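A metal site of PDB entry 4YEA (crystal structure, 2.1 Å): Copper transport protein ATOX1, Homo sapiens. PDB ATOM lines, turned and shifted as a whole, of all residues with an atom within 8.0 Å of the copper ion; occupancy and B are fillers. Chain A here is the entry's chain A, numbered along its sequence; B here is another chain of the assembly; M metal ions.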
ATOM      1  N   ASP A   8      -0.617  -7.166 -10.906  1.00  0.00           N
ATOM      2  CA  ASP A   8      -1.284  -5.894 -10.736  1.00  0.00           C
ATOM      3  C   ASP A   8      -2.361  -5.650 -11.813  1.00  0.00           C
ATOM      4  O   ASP A   8      -2.256  -4.743 -12.617  1.00  0.00           O
ATOM      5  CB  ASP A   8      -0.258  -4.765 -10.701  1.00  0.00           C
ATOM      6  CG  ASP A   8      -0.886  -3.421 -10.458  1.00  0.00           C
ATOM      7  OD1 ASP A   8      -2.061  -3.404 -10.025  1.00  0.00           O
ATOM      8  OD2 ASP A   8      -0.237  -2.394 -10.745  1.00  0.00           O
ATOM      9  N   MET A   9      -3.412  -6.452 -11.785  1.00  0.00           N
ATOM     10  CA  MET A   9      -4.534  -6.339 -12.713  1.00  0.00           C
ATOM     11  C   MET A   9      -5.567  -5.376 -12.105  1.00  0.00           C
ATOM     12  O   MET A   9      -5.916  -5.471 -10.920  1.00  0.00           O
ATOM     13  CB  MET A   9      -5.208  -7.697 -12.917  1.00  0.00           C
ATOM     14  CG  MET A   9      -4.310  -8.852 -13.297  1.00  0.00           C
ATOM     15  SD  MET A   9      -5.039 -10.473 -12.996  1.00  0.00           S
ATOM     16  CE  MET A   9      -5.126 -10.546 -11.218  1.00  0.00           C
ATOM     17  N   THR A  10      -6.036  -4.432 -12.917  1.00  0.00           N
ATOM     18  CA  THR A  10      -6.929  -3.370 -12.468  1.00  0.00           C
ATOM     19  C   THR A  10      -8.222  -3.283 -13.266  1.00  0.00           C
ATOM     20  O   THR A  10      -8.966  -2.349 -13.074  1.00  0.00           O
ATOM     21  CB  THR A  10      -6.168  -2.016 -12.505  1.00  0.00           C
ATOM     22  OG1 THR A  10      -5.524  -1.861 -13.781  1.00  0.00           O
ATOM     23  CG2 THR A  10      -5.103  -1.938 -11.369  1.00  0.00           C
ATOM     24  N   CYS A  11      -8.484  -4.237 -14.165  1.00  0.00           N
ATOM     25  CA  CYS A  11      -9.721  -4.324 -14.919  1.00  0.00           C
ATOM     26  C   CYS A  11      -9.886  -5.761 -15.405  1.00  0.00           C
ATOM     27  O   CYS A  11      -8.956  -6.559 -15.347  1.00  0.00           O
ATOM     28  CB  CYS A  11      -9.752  -3.307 -16.105  1.00  0.00           C
ATOM     29  SG  CYS A  11      -9.023  -3.815 -17.687  1.00  0.00           S
ATOM     30  N   GLY A  12     -11.068  -6.089 -15.892  1.00  0.00           N
ATOM     31  CA  GLY A  12     -11.349  -7.420 -16.416  1.00  0.00           C
ATOM     32  C   GLY A  12     -10.466  -7.769 -17.603  1.00  0.00           C
ATOM     33  O   GLY A  12     -10.069  -8.927 -17.763  1.00  0.00           O
ATOM     34  N   GLY A  13     -10.202  -6.791 -18.449  1.00  0.00           N
ATOM     35  CA  GLY A  13      -9.244  -6.915 -19.560  1.00  0.00           C
ATOM     36  C   GLY A  13      -7.848  -7.398 -19.152  1.00  0.00           C
ATOM     37  O   GLY A  13      -7.277  -8.262 -19.801  1.00  0.00           O
ATOM     38  N   CYS A  14      -7.334  -6.841 -18.059  1.00  0.00           N
ATOM     39  CA  CYS A  14      -6.050  -7.259 -17.479  1.00  0.00           C
ATOM     40  C   CYS A  14      -6.102  -8.733 -17.084  1.00  0.00           C
ATOM     41  O   CYS A  14      -5.157  -9.511 -17.376  1.00  0.00           O
ATOM     42  CB  CYS A  14      -5.670  -6.396 -16.275  1.00  0.00           C
ATOM     43  SG  CYS A  14      -5.289  -4.653 -16.605  1.00  0.00           S
ATOM     44  N   ALA A  15      -7.223  -9.150 -16.478  1.00  0.00           N
ATOM     45  CA  ALA A  15      -7.405 -10.554 -16.105  1.00  0.00           C
ATOM     46  C   ALA A  15      -7.420 -11.475 -17.298  1.00  0.00           C
ATOM     47  O   ALA A  15      -6.734 -12.511 -17.316  1.00  0.00           O
ATOM     48  CB  ALA A  15      -8.661 -10.754 -15.268  1.00  0.00           C
ATOM     49  N   GLU A  16      -8.179 -11.079 -18.319  1.00  0.00           N
ATOM     50  CA  GLU A  16      -8.263 -11.914 -19.529  1.00  0.00           C
ATOM     51  C   GLU A  16      -6.935 -12.069 -20.246  1.00  0.00           C
ATOM     52  O   GLU A  16      -6.641 -13.156 -20.816  1.00  0.00           O
ATOM     53  CB  GLU A  16      -9.325 -11.363 -20.514  1.00  0.00           C
ATOM     54  CG  GLU A  16     -10.107 -12.489 -21.173  1.00  0.00           C
ATOM     55  CD  GLU A  16     -11.172 -12.052 -22.144  1.00  0.00           C
ATOM     56  OE1 GLU A  16     -11.134 -10.882 -22.601  1.00  0.00           O
ATOM     57  OE2 GLU A  16     -12.045 -12.900 -22.471  1.00  0.00           O
ATOM     58  N   ALA A  17      -6.131 -11.015 -20.238  1.00  0.00           N
ATOM     59  CA  ALA A  17      -4.800 -11.046 -20.883  1.00  0.00           C
ATOM     60  C   ALA A  17      -3.872 -12.040 -20.167  1.00  0.00           C
ATOM     61  O   ALA A  17      -3.092 -12.742 -20.796  1.00  0.00           O
ATOM     62  CB  ALA A  17      -4.178  -9.682 -20.900  1.00  0.00           C
ATOM     63  N   LEU A  34      -9.504 -11.112  -9.503  1.00  0.00           N
ATOM     64  CA  LEU A  34      -9.246  -9.720  -9.898  1.00  0.00           C
ATOM     65  C   LEU A  34      -9.157  -8.781  -8.661  1.00  0.00           C
ATOM     66  O   LEU A  34      -8.150  -8.056  -8.521  1.00  0.00           O
ATOM     67  CB  LEU A  34     -10.231  -9.209 -10.994  1.00  0.00           C
ATOM     68  CG  LEU A  34     -10.107  -7.730 -11.461  1.00  0.00           C
ATOM     69  CD1 LEU A  34      -8.710  -7.388 -11.975  1.00  0.00           C
ATOM     70  CD2 LEU A  34     -11.132  -7.371 -12.521  1.00  0.00           C
ATOM     71  N   LYS A  59       2.533  -6.486 -17.013  1.00  0.00           N
ATOM     72  CA  LYS A  59       2.028  -6.147 -15.678  1.00  0.00           C
ATOM     73  C   LYS A  59       3.132  -6.415 -14.643  1.00  0.00           C
ATOM     74  O   LYS A  59       4.011  -7.239 -14.870  1.00  0.00           O
ATOM     75  CB  LYS A  59       0.832  -7.026 -15.311  1.00  0.00           C
ATOM     76  CG  LYS A  59      -0.370  -6.908 -16.224  1.00  0.00           C
ATOM     77  CD  LYS A  59      -1.411  -5.939 -15.649  1.00  0.00           C
ATOM     78  CE  LYS A  59      -1.116  -4.477 -16.000  1.00  0.00           C
ATOM     79  NZ  LYS A  59      -1.846  -3.527 -15.104  1.00  0.00           N
ATOM     80  N   ASP B   8      -6.607  -3.835 -27.788  1.00  0.00           N
ATOM     81  CA  ASP B   8      -7.846  -3.797 -27.033  1.00  0.00           C
ATOM     82  C   ASP B   8      -7.495  -3.561 -25.562  1.00  0.00           C
ATOM     83  O   ASP B   8      -7.241  -4.506 -24.815  1.00  0.00           O
ATOM     84  CB  ASP B   8      -8.568  -5.123 -27.255  1.00  0.00           C
ATOM     85  CG  ASP B   8      -9.786  -5.267 -26.408  1.00  0.00           C
ATOM     86  OD1 ASP B   8     -10.461  -4.285 -26.070  1.00  0.00           O
ATOM     87  OD2 ASP B   8     -10.059  -6.409 -26.037  1.00  0.00           O
ATOM     88  N   MET B   9      -7.366  -2.304 -25.197  1.00  0.00           N
ATOM     89  CA  MET B   9      -6.987  -1.886 -23.886  1.00  0.00           C
ATOM     90  C   MET B   9      -8.257  -1.282 -23.320  1.00  0.00           C
ATOM     91  O   MET B   9      -8.973  -0.548 -24.022  1.00  0.00           O
ATOM     92  CB  MET B   9      -5.921  -0.797 -23.952  1.00  0.00           C
ATOM     93  CG  MET B   9      -4.610  -1.152 -24.629  1.00  0.00           C
ATOM     94  SD  MET B   9      -3.633   0.337 -25.020  1.00  0.00           S
ATOM     95  CE  MET B   9      -4.573   1.031 -26.371  1.00  0.00           C
ATOM     96  N   THR B  10      -8.530  -1.591 -22.060  1.00  0.00           N
ATOM     97  CA  THR B  10      -9.751  -1.102 -21.464  1.00  0.00           C
ATOM     98  C   THR B  10      -9.493  -0.190 -20.281  1.00  0.00           C
ATOM     99  O   THR B  10     -10.352   0.563 -19.936  1.00  0.00           O
ATOM    100  CB  THR B  10     -10.749  -2.258 -21.155  1.00  0.00           C
ATOM    101  OG1 THR B  10     -10.069  -3.373 -20.628  1.00  0.00           O
ATOM    102  CG2 THR B  10     -11.378  -2.753 -22.437  1.00  0.00           C
ATOM    103  N   CYS B  11      -8.329  -0.211 -19.669  1.00  0.00           N
ATOM    104  CA  CYS B  11      -8.032   0.682 -18.541  1.00  0.00           C
ATOM    105  C   CYS B  11      -6.622   1.211 -18.691  1.00  0.00           C
ATOM    106  O   CYS B  11      -5.873   0.781 -19.542  1.00  0.00           O
ATOM    107  CB  CYS B  11      -8.226  -0.047 -17.192  1.00  0.00           C
ATOM    108  SG  CYS B  11      -6.938  -1.225 -16.718  1.00  0.00           S
ATOM    109  N   GLY B  12      -6.290   2.183 -17.862  1.00  0.00           N
ATOM    110  CA  GLY B  12      -4.960   2.732 -17.814  1.00  0.00           C
ATOM    111  C   GLY B  12      -3.895   1.707 -17.524  1.00  0.00           C
ATOM    112  O   GLY B  12      -2.802   1.812 -18.056  1.00  0.00           O
ATOM    113  N   GLY B  13      -4.199   0.721 -16.675  1.00  0.00           N
ATOM    114  CA  GLY B  13      -3.331  -0.459 -16.472  1.00  0.00           C
ATOM    115  C   GLY B  13      -2.938  -1.199 -17.755  1.00  0.00           C
ATOM    116  O   GLY B  13      -1.794  -1.698 -17.887  1.00  0.00           O
ATOM    117  N   CYS B  14      -3.881  -1.312 -18.686  1.00  0.00           N
ATOM    118  CA  CYS B  14      -3.640  -1.937 -19.978  1.00  0.00           C
ATOM    119  C   CYS B  14      -2.684  -1.077 -20.823  1.00  0.00           C
ATOM    120  O   CYS B  14      -1.765  -1.600 -21.503  1.00  0.00           O
ATOM    121  CB  CYS B  14      -4.917  -2.144 -20.753  1.00  0.00           C
ATOM    122  SG  CYS B  14      -6.107  -3.238 -20.029  1.00  0.00           S
ATOM    123  N   ALA B  15      -2.901   0.227 -20.771  1.00  0.00           N
ATOM    124  CA  ALA B  15      -1.988   1.161 -21.436  1.00  0.00           C
ATOM    125  C   ALA B  15      -0.546   1.106 -20.895  1.00  0.00           C
ATOM    126  O   ALA B  15       0.431   1.198 -21.683  1.00  0.00           O
ATOM    127  CB  ALA B  15      -2.537   2.553 -21.369  1.00  0.00           C
ATOM    128  N   GLU B  16      -0.419   0.974 -19.567  1.00  0.00           N
ATOM    129  CA  GLU B  16       0.874   0.853 -18.932  1.00  0.00           C
ATOM    130  C   GLU B  16       1.577  -0.401 -19.380  1.00  0.00           C
ATOM    131  O   GLU B  16       2.752  -0.360 -19.629  1.00  0.00           O
ATOM    132  CB  GLU B  16       0.750   0.840 -17.413  1.00  0.00           C
ATOM    133  CG  GLU B  16       0.349   2.188 -16.848  1.00  0.00           C
ATOM    134  CD  GLU B  16       0.074   2.147 -15.360  1.00  0.00           C
ATOM    135  OE1 GLU B  16       0.040   1.055 -14.778  1.00  0.00           O
ATOM    136  OE2 GLU B  16      -0.140   3.192 -14.764  1.00  0.00           O
ATOM    137  N   ALA B  17       0.824  -1.494 -19.480  1.00  0.00           N
ATOM    138  CA  ALA B  17       1.370  -2.790 -19.887  1.00  0.00           C
ATOM    139  C   ALA B  17       1.975  -2.748 -21.291  1.00  0.00           C
ATOM    140  O   ALA B  17       3.085  -3.245 -21.534  1.00  0.00           O
ATOM    141  CB  ALA B  17       0.265  -3.838 -19.841  1.00  0.00           C
ATOM    142  N   LEU B  34      -5.639   5.495 -25.467  1.00  0.00           N
ATOM    143  CA  LEU B  34      -6.455   4.526 -24.730  1.00  0.00           C
ATOM    144  C   LEU B  34      -7.951   4.465 -25.166  1.00  0.00           C
ATOM    145  O   LEU B  34      -8.433   3.389 -25.490  1.00  0.00           O
ATOM    146  CB  LEU B  34      -6.281   4.732 -23.218  1.00  0.00           C
ATOM    147  CG  LEU B  34      -7.160   3.908 -22.267  1.00  0.00           C
ATOM    148  CD1 LEU B  34      -6.864   2.428 -22.475  1.00  0.00           C
ATOM    149  CD2 LEU B  34      -6.898   4.295 -20.822  1.00  0.00           C
ATOM    150  N   LYS B  59      -3.285  -9.275 -25.054  1.00  0.00           N
ATOM    151  CA  LYS B  59      -4.403  -8.462 -25.532  1.00  0.00           C
ATOM    152  C   LYS B  59      -4.625  -8.726 -27.010  1.00  0.00           C
ATOM    153  O   LYS B  59      -3.693  -9.152 -27.727  1.00  0.00           O
ATOM    154  CB  LYS B  59      -4.112  -6.990 -25.308  1.00  0.00           C
ATOM    155  CG  LYS B  59      -3.899  -6.652 -23.840  1.00  0.00           C
ATOM    156  CD  LYS B  59      -3.371  -5.259 -23.641  1.00  0.00           C
ATOM    157  CE  LYS B  59      -2.796  -5.052 -22.244  1.00  0.00           C
ATOM    158  NZ  LYS B  59      -3.579  -5.728 -21.145  1.00  0.00           N
HETATM  159 CU    CU M   1      -6.757  -3.275 -17.798  1.00  0.00          CU
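N of Gly 13 of chain B lies close to SG of Cys 11 of chain B (3.4 Å).
The side-chain sulfur of Cys 14 of chain A sits close to the backbone NH of Thr 10 of chain A.
SG of Cys 14 of chain B lies close to NZ of Lys 59 of chain B (3.7 Å).
The side-chain sulfur (SG) of Cys 14 of chain B lies close to the backbone NH (N) of Thr 10 of chain B.
SG of Cys 11 of chain A sits close to N of Gly 13 of chain A (3.3 Å).
SG of Cys 11 of chain B lies close to OG1 of Thr 10 of chain A, 3.3 Å away.
The side-chain sulfur (SG) of Cys 11 of chain A sits close to the side-chain hydroxyl (OG1) of Thr 10 of chain B (3.2 Å).
The nearest printed residue that does not touch the copper ion is Gly 13 of chain B (4.3 Å).
The copper ion is bound by SG of Cys 14 of chain B (2.3 Å), SG of Cys 11 of chain B (2.3 Å), SG of Cys 11 of chain A (2.3 Å) and SG of Cys 14 of chain A (2.3 Å).
The copper ion has four donor atoms within binding distance.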
